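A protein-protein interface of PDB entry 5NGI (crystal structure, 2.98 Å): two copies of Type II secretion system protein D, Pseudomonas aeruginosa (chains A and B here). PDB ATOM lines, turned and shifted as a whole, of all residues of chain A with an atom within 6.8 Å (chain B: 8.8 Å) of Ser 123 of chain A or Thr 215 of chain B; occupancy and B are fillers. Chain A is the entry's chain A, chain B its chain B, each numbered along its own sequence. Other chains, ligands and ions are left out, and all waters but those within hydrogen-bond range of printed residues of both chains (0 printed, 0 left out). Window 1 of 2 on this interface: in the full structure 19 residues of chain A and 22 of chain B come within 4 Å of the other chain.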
ATOM      1  N   SER A 120      13.012  -0.120  17.938  1.00  0.00           N
ATOM      2  CA  SER A 120      13.562  -1.472  18.154  1.00  0.00           C
ATOM      3  C   SER A 120      14.103  -2.157  16.861  1.00  0.00           C
ATOM      4  O   SER A 120      13.638  -1.789  15.779  1.00  0.00           O
ATOM      5  CB  SER A 120      12.495  -2.358  18.805  1.00  0.00           C
ATOM      6  OG  SER A 120      11.220  -2.249  18.184  1.00  0.00           O
ATOM      7  N   PRO A 121      15.037  -3.164  16.905  1.00  0.00           N
ATOM      8  CA  PRO A 121      15.396  -3.878  15.654  1.00  0.00           C
ATOM      9  C   PRO A 121      14.160  -4.589  15.076  1.00  0.00           C
ATOM     10  O   PRO A 121      13.294  -5.011  15.848  1.00  0.00           O
ATOM     11  CB  PRO A 121      16.469  -4.894  16.092  1.00  0.00           C
ATOM     12  CG  PRO A 121      16.851  -4.510  17.461  1.00  0.00           C
ATOM     13  CD  PRO A 121      15.680  -3.805  18.066  1.00  0.00           C
ATOM     14  N   VAL A 122      14.041  -4.678  13.738  1.00  0.00           N
ATOM     15  CA  VAL A 122      12.893  -5.298  13.055  1.00  0.00           C
ATOM     16  C   VAL A 122      12.588  -6.699  13.530  1.00  0.00           C
ATOM     17  O   VAL A 122      11.416  -7.036  13.688  1.00  0.00           O
ATOM     18  CB  VAL A 122      12.965  -5.273  11.520  1.00  0.00           C
ATOM     19  CG1 VAL A 122      12.331  -4.021  10.975  1.00  0.00           C
ATOM     20  CG2 VAL A 122      14.385  -5.452  11.000  1.00  0.00           C
ATOM     21  N   SER A 123      13.637  -7.515  13.760  1.00  0.00           N
ATOM     22  CA  SER A 123      13.534  -8.896  14.243  1.00  0.00           C
ATOM     23  C   SER A 123      12.567  -9.024  15.426  1.00  0.00           C
ATOM     24  O   SER A 123      11.774  -9.970  15.462  1.00  0.00           O
ATOM     25  CB  SER A 123      14.911  -9.413  14.637  1.00  0.00           C
ATOM     26  OG  SER A 123      15.514  -8.549  15.584  1.00  0.00           O
ATOM     27  N   GLU A 124      12.587  -8.021  16.338  1.00  0.00           N
ATOM     28  CA  GLU A 124      11.737  -7.913  17.518  1.00  0.00           C
ATOM     29  C   GLU A 124      10.244  -7.809  17.188  1.00  0.00           C
ATOM     30  O   GLU A 124       9.447  -8.361  17.940  1.00  0.00           O
ATOM     31  CB  GLU A 124      12.160  -6.713  18.380  1.00  0.00           C
ATOM     32  CG  GLU A 124      13.558  -6.823  18.981  1.00  0.00           C
ATOM     33  CD  GLU A 124      13.835  -6.083  20.279  1.00  0.00           C
ATOM     34  OE1 GLU A 124      12.883  -5.559  20.900  1.00  0.00           O
ATOM     35  OE2 GLU A 124      15.020  -6.037  20.679  1.00  0.00           O
ATOM     36  N   LEU A 125       9.855  -7.099  16.096  1.00  0.00           N
ATOM     37  CA  LEU A 125       8.445  -6.880  15.707  1.00  0.00           C
ATOM     38  C   LEU A 125       7.869  -7.857  14.675  1.00  0.00           C
ATOM     39  O   LEU A 125       6.649  -7.881  14.492  1.00  0.00           O
ATOM     40  CB  LEU A 125       8.209  -5.443  15.212  1.00  0.00           C
ATOM     41  CG  LEU A 125       8.565  -4.285  16.125  1.00  0.00           C
ATOM     42  CD1 LEU A 125       8.071  -3.009  15.532  1.00  0.00           C
ATOM     43  CD2 LEU A 125       7.962  -4.451  17.505  1.00  0.00           C
ATOM     44  N   ILE A 126       8.723  -8.617  13.961  1.00  0.00           N
ATOM     45  CA  ILE A 126       8.250  -9.602  12.977  1.00  0.00           C
ATOM     46  C   ILE A 126       7.278 -10.634  13.658  1.00  0.00           C
ATOM     47  O   ILE A 126       6.136 -10.721  13.194  1.00  0.00           O
ATOM     48  CB  ILE A 126       9.421 -10.277  12.166  1.00  0.00           C
ATOM     49  CG1 ILE A 126      10.244  -9.266  11.294  1.00  0.00           C
ATOM     50  CG2 ILE A 126       8.944 -11.467  11.329  1.00  0.00           C
ATOM     51  CD1 ILE A 126       9.602  -8.699  10.021  1.00  0.00           C
ATOM     52  N   PRO A 127       7.655 -11.354  14.769  1.00  0.00           N
ATOM     53  CA  PRO A 127       6.726 -12.337  15.366  1.00  0.00           C
ATOM     54  C   PRO A 127       5.363 -11.799  15.806  1.00  0.00           C
ATOM     55  O   PRO A 127       4.363 -12.545  15.831  1.00  0.00           O
ATOM     56  CB  PRO A 127       7.513 -12.880  16.560  1.00  0.00           C
ATOM     57  CG  PRO A 127       8.929 -12.678  16.195  1.00  0.00           C
ATOM     58  CD  PRO A 127       8.956 -11.384  15.473  1.00  0.00           C
ATOM     59  N   LEU A 128       5.328 -10.504  16.151  1.00  0.00           N
ATOM     60  CA  LEU A 128       4.136  -9.820  16.633  1.00  0.00           C
ATOM     61  C   LEU A 128       3.198  -9.350  15.502  1.00  0.00           C
ATOM     62  O   LEU A 128       1.978  -9.290  15.702  1.00  0.00           O
ATOM     63  CB  LEU A 128       4.500  -8.656  17.592  1.00  0.00           C
ATOM     64  CG  LEU A 128       5.636  -8.873  18.614  1.00  0.00           C
ATOM     65  CD1 LEU A 128       6.146  -7.557  19.165  1.00  0.00           C
ATOM     66  CD2 LEU A 128       5.226  -9.811  19.734  1.00  0.00           C
ATOM     67  N   ALA A 141      11.957  -9.110   6.358  1.00  0.00           N
ATOM     68  CA  ALA A 141      12.784  -8.034   6.886  1.00  0.00           C
ATOM     69  C   ALA A 141      13.933  -7.660   5.970  1.00  0.00           C
ATOM     70  O   ALA A 141      14.451  -8.501   5.228  1.00  0.00           O
ATOM     71  CB  ALA A 141      13.323  -8.414   8.250  1.00  0.00           C
ATOM     72  N   ASN A 146      16.650  -1.849   8.557  1.00  0.00           N
ATOM     73  CA  ASN A 146      15.840  -2.026   9.772  1.00  0.00           C
ATOM     74  C   ASN A 146      14.398  -1.710   9.438  1.00  0.00           C
ATOM     75  O   ASN A 146      13.730  -0.919  10.100  1.00  0.00           O
ATOM     76  CB  ASN A 146      16.350  -1.192  10.951  1.00  0.00           C
ATOM     77  CG  ASN A 146      15.892  -1.729  12.275  1.00  0.00           C
ATOM     78  OD1 ASN A 146      16.250  -2.844  12.661  1.00  0.00           O
ATOM     79  ND2 ASN A 146      15.078  -0.964  12.997  1.00  0.00           N
ATOM     80  N   TYR A 175       8.046 -11.674  24.669  1.00  0.00           N
ATOM     81  CA  TYR A 175       6.680 -12.163  24.603  1.00  0.00           C
ATOM     82  C   TYR A 175       6.518 -13.610  25.022  1.00  0.00           C
ATOM     83  O   TYR A 175       7.487 -14.362  25.081  1.00  0.00           O
ATOM     84  CB  TYR A 175       6.126 -11.935  23.180  1.00  0.00           C
ATOM     85  CG  TYR A 175       6.791 -12.743  22.084  1.00  0.00           C
ATOM     86  CD1 TYR A 175       7.871 -12.236  21.377  1.00  0.00           C
ATOM     87  CD2 TYR A 175       6.283 -13.981  21.690  1.00  0.00           C
ATOM     88  CE1 TYR A 175       8.471 -12.963  20.356  1.00  0.00           C
ATOM     89  CE2 TYR A 175       6.883 -14.726  20.679  1.00  0.00           C
ATOM     90  CZ  TYR A 175       7.959 -14.200  19.991  1.00  0.00           C
ATOM     91  OH  TYR A 175       8.537 -14.935  18.976  1.00  0.00           O
ATOM     92  N   ARG B 130      13.272 -23.202  14.080  1.00  0.00           N
ATOM     93  CA  ARG B 130      13.711 -22.068  13.242  1.00  0.00           C
ATOM     94  C   ARG B 130      15.017 -21.432  13.751  1.00  0.00           C
ATOM     95  O   ARG B 130      15.918 -21.260  12.934  1.00  0.00           O
ATOM     96  CB  ARG B 130      12.596 -21.020  13.066  1.00  0.00           C
ATOM     97  CG  ARG B 130      12.852 -20.055  11.917  1.00  0.00           C
ATOM     98  CD  ARG B 130      11.638 -19.200  11.560  1.00  0.00           C
ATOM     99  NE  ARG B 130      10.587 -19.910  10.816  1.00  0.00           N
ATOM    100  CZ  ARG B 130      10.667 -20.259   9.529  1.00  0.00           C
ATOM    101  NH1 ARG B 130      11.781 -20.031   8.835  1.00  0.00           N
ATOM    102  NH2 ARG B 130       9.651 -20.881   8.940  1.00  0.00           N
ATOM    103  N   PRO B 131      15.191 -21.185  15.092  1.00  0.00           N
ATOM    104  CA  PRO B 131      16.456 -20.618  15.586  1.00  0.00           C
ATOM    105  C   PRO B 131      17.710 -21.468  15.370  1.00  0.00           C
ATOM    106  O   PRO B 131      18.791 -20.883  15.298  1.00  0.00           O
ATOM    107  CB  PRO B 131      16.165 -20.399  17.068  1.00  0.00           C
ATOM    108  CG  PRO B 131      14.657 -20.205  17.110  1.00  0.00           C
ATOM    109  CD  PRO B 131      14.226 -21.290  16.210  1.00  0.00           C
ATOM    110  N   VAL B 133      18.430 -22.930  12.606  1.00  0.00           N
ATOM    111  CA  VAL B 133      18.594 -22.906  11.160  1.00  0.00           C
ATOM    112  C   VAL B 133      19.452 -21.682  10.758  1.00  0.00           C
ATOM    113  O   VAL B 133      19.168 -20.559  11.198  1.00  0.00           O
ATOM    114  CB  VAL B 133      17.227 -23.048  10.411  1.00  0.00           C
ATOM    115  CG1 VAL B 133      16.867 -21.840   9.545  1.00  0.00           C
ATOM    116  CG2 VAL B 133      17.187 -24.326   9.598  1.00  0.00           C
ATOM    117  N   VAL B 177       9.904 -15.821  24.899  1.00  0.00           N
ATOM    118  CA  VAL B 177      11.030 -15.234  24.173  1.00  0.00           C
ATOM    119  C   VAL B 177      11.624 -14.079  24.938  1.00  0.00           C
ATOM    120  O   VAL B 177      10.893 -13.173  25.365  1.00  0.00           O
ATOM    121  CB  VAL B 177      10.645 -14.817  22.749  1.00  0.00           C
ATOM    122  CG1 VAL B 177      11.818 -14.174  22.025  1.00  0.00           C
ATOM    123  CG2 VAL B 177      10.116 -16.012  21.971  1.00  0.00           C
ATOM    124  N   ILE B 178      12.958 -14.125  25.108  1.00  0.00           N
ATOM    125  CA  ILE B 178      13.712 -13.065  25.746  1.00  0.00           C
ATOM    126  C   ILE B 178      14.685 -12.498  24.726  1.00  0.00           C
ATOM    127  O   ILE B 178      15.590 -13.195  24.267  1.00  0.00           O
ATOM    128  CB  ILE B 178      14.398 -13.482  27.082  1.00  0.00           C
ATOM    129  CG1 ILE B 178      13.394 -14.124  28.065  1.00  0.00           C
ATOM    130  CG2 ILE B 178      15.101 -12.287  27.742  1.00  0.00           C
ATOM    131  CD1 ILE B 178      13.887 -15.408  28.637  1.00  0.00           C
ATOM    132  N   ASN B 179      14.464 -11.231  24.366  1.00  0.00           N
ATOM    133  CA  ASN B 179      15.315 -10.457  23.466  1.00  0.00           C
ATOM    134  C   ASN B 179      16.427  -9.864  24.340  1.00  0.00           C
ATOM    135  O   ASN B 179      16.160  -8.912  25.087  1.00  0.00           O
ATOM    136  CB  ASN B 179      14.507  -9.326  22.818  1.00  0.00           C
ATOM    137  CG  ASN B 179      13.470  -9.759  21.821  1.00  0.00           C
ATOM    138  OD1 ASN B 179      13.661 -10.694  21.033  1.00  0.00           O
ATOM    139  ND2 ASN B 179      12.370  -9.025  21.786  1.00  0.00           N
ATOM    140  N   LEU B 180      17.652 -10.445  24.302  1.00  0.00           N
ATOM    141  CA  LEU B 180      18.765  -9.955  25.148  1.00  0.00           C
ATOM    142  C   LEU B 180      19.431  -8.712  24.596  1.00  0.00           C
ATOM    143  O   LEU B 180      19.660  -8.607  23.394  1.00  0.00           O
ATOM    144  CB  LEU B 180      19.824 -11.031  25.426  1.00  0.00           C
ATOM    145  CG  LEU B 180      19.380 -12.220  26.247  1.00  0.00           C
ATOM    146  CD1 LEU B 180      20.241 -13.408  25.954  1.00  0.00           C
ATOM    147  CD2 LEU B 180      19.375 -11.897  27.734  1.00  0.00           C
ATOM    148  N   ARG B 181      19.728  -7.768  25.468  1.00  0.00           N
ATOM    149  CA  ARG B 181      20.389  -6.537  25.068  1.00  0.00           C
ATOM    150  C   ARG B 181      21.742  -6.381  25.793  1.00  0.00           C
ATOM    151  O   ARG B 181      22.763  -6.213  25.121  1.00  0.00           O
ATOM    152  CB  ARG B 181      19.461  -5.300  25.202  1.00  0.00           C
ATOM    153  CG  ARG B 181      18.927  -4.981  26.613  1.00  0.00           C
ATOM    154  CD  ARG B 181      17.463  -5.344  26.780  1.00  0.00           C
ATOM    155  N   GLY B 183      23.431  -8.726  27.267  1.00  0.00           N
ATOM    156  CA  GLY B 183      24.212  -9.952  27.175  1.00  0.00           C
ATOM    157  C   GLY B 183      24.411 -10.529  25.790  1.00  0.00           C
ATOM    158  O   GLY B 183      24.105  -9.893  24.778  1.00  0.00           O
ATOM    159  N   TRP B 184      24.951 -11.751  25.761  1.00  0.00           N
ATOM    160  CA  TRP B 184      25.220 -12.531  24.566  1.00  0.00           C
ATOM    161  C   TRP B 184      24.591 -13.895  24.781  1.00  0.00           C
ATOM    162  O   TRP B 184      24.907 -14.595  25.747  1.00  0.00           O
ATOM    163  CB  TRP B 184      26.722 -12.607  24.290  1.00  0.00           C
ATOM    164  CG  TRP B 184      27.112 -13.592  23.229  1.00  0.00           C
ATOM    165  CD1 TRP B 184      27.824 -14.743  23.403  1.00  0.00           C
ATOM    166  CD2 TRP B 184      26.808 -13.517  21.836  1.00  0.00           C
ATOM    167  NE1 TRP B 184      27.999 -15.381  22.199  1.00  0.00           N
ATOM    168  CE2 TRP B 184      27.362 -14.664  21.223  1.00  0.00           C
ATOM    169  CE3 TRP B 184      26.116 -12.592  21.039  1.00  0.00           C
ATOM    170  CZ2 TRP B 184      27.257 -14.903  19.849  1.00  0.00           C
ATOM    171  CZ3 TRP B 184      26.004 -12.833  19.679  1.00  0.00           C
ATOM    172  CH2 TRP B 184      26.572 -13.976  19.096  1.00  0.00           C
ATOM    173  N   VAL B 185      23.649 -14.225  23.895  1.00  0.00           N
ATOM    174  CA  VAL B 185      22.780 -15.396  23.897  1.00  0.00           C
ATOM    175  C   VAL B 185      23.513 -16.741  24.139  1.00  0.00           C
ATOM    176  O   VAL B 185      23.047 -17.503  24.985  1.00  0.00           O
ATOM    177  CB  VAL B 185      21.887 -15.423  22.624  1.00  0.00           C
ATOM    178  CG1 VAL B 185      22.681 -15.588  21.329  1.00  0.00           C
ATOM    179  CG2 VAL B 185      20.799 -16.467  22.729  1.00  0.00           C
ATOM    180  N   ILE B 210      16.591 -22.430  24.159  1.00  0.00           N
ATOM    181  CA  ILE B 210      17.005 -22.402  22.762  1.00  0.00           C
ATOM    182  C   ILE B 210      17.620 -21.025  22.492  1.00  0.00           C
ATOM    183  O   ILE B 210      17.046 -20.005  22.868  1.00  0.00           O
ATOM    184  CB  ILE B 210      15.867 -22.809  21.784  1.00  0.00           C
ATOM    185  CG1 ILE B 210      15.512 -24.314  21.945  1.00  0.00           C
ATOM    186  CG2 ILE B 210      16.226 -22.472  20.313  1.00  0.00           C
ATOM    187  CD1 ILE B 210      14.228 -24.800  21.216  1.00  0.00           C
ATOM    188  N   ALA B 211      18.825 -21.016  21.897  1.00  0.00           N
ATOM    189  CA  ALA B 211      19.575 -19.809  21.590  1.00  0.00           C
ATOM    190  C   ALA B 211      19.483 -19.457  20.114  1.00  0.00           C
ATOM    191  O   ALA B 211      19.755 -20.305  19.269  1.00  0.00           O
ATOM    192  CB  ALA B 211      21.028 -19.995  21.995  1.00  0.00           C
ATOM    193  N   ASP B 212      19.067 -18.216  19.795  1.00  0.00           N
ATOM    194  CA  ASP B 212      19.001 -17.719  18.415  1.00  0.00           C
ATOM    195  C   ASP B 212      20.016 -16.591  18.352  1.00  0.00           C
ATOM    196  O   ASP B 212      19.749 -15.481  18.835  1.00  0.00           O
ATOM    197  CB  ASP B 212      17.585 -17.232  18.024  1.00  0.00           C
ATOM    198  CG  ASP B 212      17.317 -17.033  16.530  1.00  0.00           C
ATOM    199  OD1 ASP B 212      18.297 -16.907  15.751  1.00  0.00           O
ATOM    200  OD2 ASP B 212      16.124 -16.955  16.146  1.00  0.00           O
ATOM    201  N   ALA B 213      21.213 -16.906  17.832  1.00  0.00           N
ATOM    202  CA  ALA B 213      22.318 -15.959  17.741  1.00  0.00           C
ATOM    203  C   ALA B 213      22.066 -14.829  16.751  1.00  0.00           C
ATOM    204  O   ALA B 213      22.435 -13.676  17.036  1.00  0.00           O
ATOM    205  CB  ALA B 213      23.600 -16.692  17.406  1.00  0.00           C
ATOM    206  N   ARG B 214      21.425 -15.161  15.602  1.00  0.00           N
ATOM    207  CA  ARG B 214      21.081 -14.233  14.520  1.00  0.00           C
ATOM    208  C   ARG B 214      20.324 -13.015  15.058  1.00  0.00           C
ATOM    209  O   ARG B 214      20.776 -11.882  14.876  1.00  0.00           O
ATOM    210  CB  ARG B 214      20.277 -14.955  13.422  1.00  0.00           C
ATOM    211  N   THR B 215      19.234 -13.266  15.803  1.00  0.00           N
ATOM    212  CA  THR B 215      18.370 -12.245  16.404  1.00  0.00           C
ATOM    213  C   THR B 215      18.759 -11.879  17.862  1.00  0.00           C
ATOM    214  O   THR B 215      18.181 -10.936  18.411  1.00  0.00           O
ATOM    215  CB  THR B 215      16.890 -12.696  16.289  1.00  0.00           C
ATOM    216  OG1 THR B 215      16.760 -14.002  16.847  1.00  0.00           O
ATOM    217  CG2 THR B 215      16.393 -12.737  14.842  1.00  0.00           C
ATOM    218  N   ASN B 216      19.733 -12.608  18.478  1.00  0.00           N
ATOM    219  CA  ASN B 216      20.195 -12.435  19.868  1.00  0.00           C
ATOM    220  C   ASN B 216      19.024 -12.526  20.860  1.00  0.00           C
ATOM    221  O   ASN B 216      18.673 -11.552  21.549  1.00  0.00           O
ATOM    222  CB  ASN B 216      21.056 -11.166  20.080  1.00  0.00           C
ATOM    223  CG  ASN B 216      21.865 -11.174  21.370  1.00  0.00           C
ATOM    224  OD1 ASN B 216      22.508 -12.164  21.747  1.00  0.00           O
ATOM    225  ND2 ASN B 216      21.889 -10.050  22.060  1.00  0.00           N
ATOM    226  N   ARG B 217      18.404 -13.717  20.891  1.00  0.00           N
ATOM    227  CA  ARG B 217      17.261 -13.990  21.748  1.00  0.00           C
ATOM    228  C   ARG B 217      17.252 -15.411  22.281  1.00  0.00           C
ATOM    229  O   ARG B 217      17.782 -16.315  21.627  1.00  0.00           O
ATOM    230  CB  ARG B 217      15.944 -13.655  21.012  1.00  0.00           C
ATOM    231  CG  ARG B 217      15.595 -14.602  19.875  1.00  0.00           C
ATOM    232  CD  ARG B 217      14.361 -14.198  19.107  1.00  0.00           C
ATOM    233  NE  ARG B 217      13.926 -15.307  18.260  1.00  0.00           N
ATOM    234  CZ  ARG B 217      12.668 -15.523  17.895  1.00  0.00           C
ATOM    235  NH1 ARG B 217      12.366 -16.568  17.139  1.00  0.00           N
ATOM    236  NH2 ARG B 217      11.703 -14.697  18.281  1.00  0.00           N
ATOM    237  N   LEU B 218      16.599 -15.604  23.446  1.00  0.00           N
ATOM    238  CA  LEU B 218      16.420 -16.899  24.099  1.00  0.00           C
ATOM    239  C   LEU B 218      14.980 -17.367  23.988  1.00  0.00           C
ATOM    240  O   LEU B 218      14.059 -16.578  24.191  1.00  0.00           O
ATOM    241  CB  LEU B 218      16.794 -16.844  25.590  1.00  0.00           C
ATOM    242  CG  LEU B 218      18.263 -16.638  25.957  1.00  0.00           C
ATOM    243  CD1 LEU B 218      18.404 -16.347  27.416  1.00  0.00           C
ATOM    244  CD2 LEU B 218      19.093 -17.844  25.663  1.00  0.00           C
ATOM    245  N   ILE B 219      14.793 -18.659  23.701  1.00  0.00           N
ATOM    246  CA  ILE B 219      13.490 -19.310  23.671  1.00  0.00           C
ATOM    247  C   ILE B 219      13.437 -20.234  24.919  1.00  0.00           C
ATOM    248  O   ILE B 219      14.317 -21.093  25.103  1.00  0.00           O
ATOM    249  CB  ILE B 219      13.193 -20.044  22.320  1.00  0.00           C
ATOM    250  CG1 ILE B 219      13.001 -19.038  21.156  1.00  0.00           C
ATOM    251  CG2 ILE B 219      11.980 -20.982  22.421  1.00  0.00           C
ATOM    252  CD1 ILE B 219      14.324 -18.692  20.338  1.00  0.00           C
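No position is printed for both chains. Of the 4 pairs that touch across the chains among the printed residues, none has its exchanged pair printed and touching as well.
O of Tyr 175 of chain A lies within hydrogen-bond range of N of Val 177 of chain B, at 2.8 Å. OH of Tyr 175 of chain A sits at hydrogen-bond distance from NH2 of Arg 217 of chain B, 3.3 Å away.
OG1 of Thr 215 of chain B sits close to OD2 of Asp 212 of chain B (3.1 Å). The guanidinium group (NE) of Arg 217 of chain B lies within salt-bridge range of the side-chain carboxylate (OD2) of Asp 212 of chain B (3.5 Å). OG1 of Thr 215 of chain B sits close to NE of Arg 217 of chain B (3.4 Å).
Among the printed residues, merely in contact across the chains: Ser 123 of chain A with Thr 215 of chain B (3.6 Å) and Glu 124 of chain A with Asn 179 of chain B (3.6 Å).
Printed residues of chain B that touch a printed residue of chain A: Val 177, Asn 179, Thr 215 and Arg 217. Hydrophobic or aromatic side chains of chain A that line the printed part of chain B: Tyr 175. Among the printed residues, 4 pairs touch across the chains.
No residue of chain B comes within 4 Å of Val 122 of chain A. Of the printed residues of chain B, Tyr 175 of chain A touches Val 177 (2.8 Å) and Arg 217 (3.3 Å). Thr 215 of chain B touches one residue of chain A. Of the printed residues of chain A, Arg 217 of chain B touches Tyr 175 (3.3 Å).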
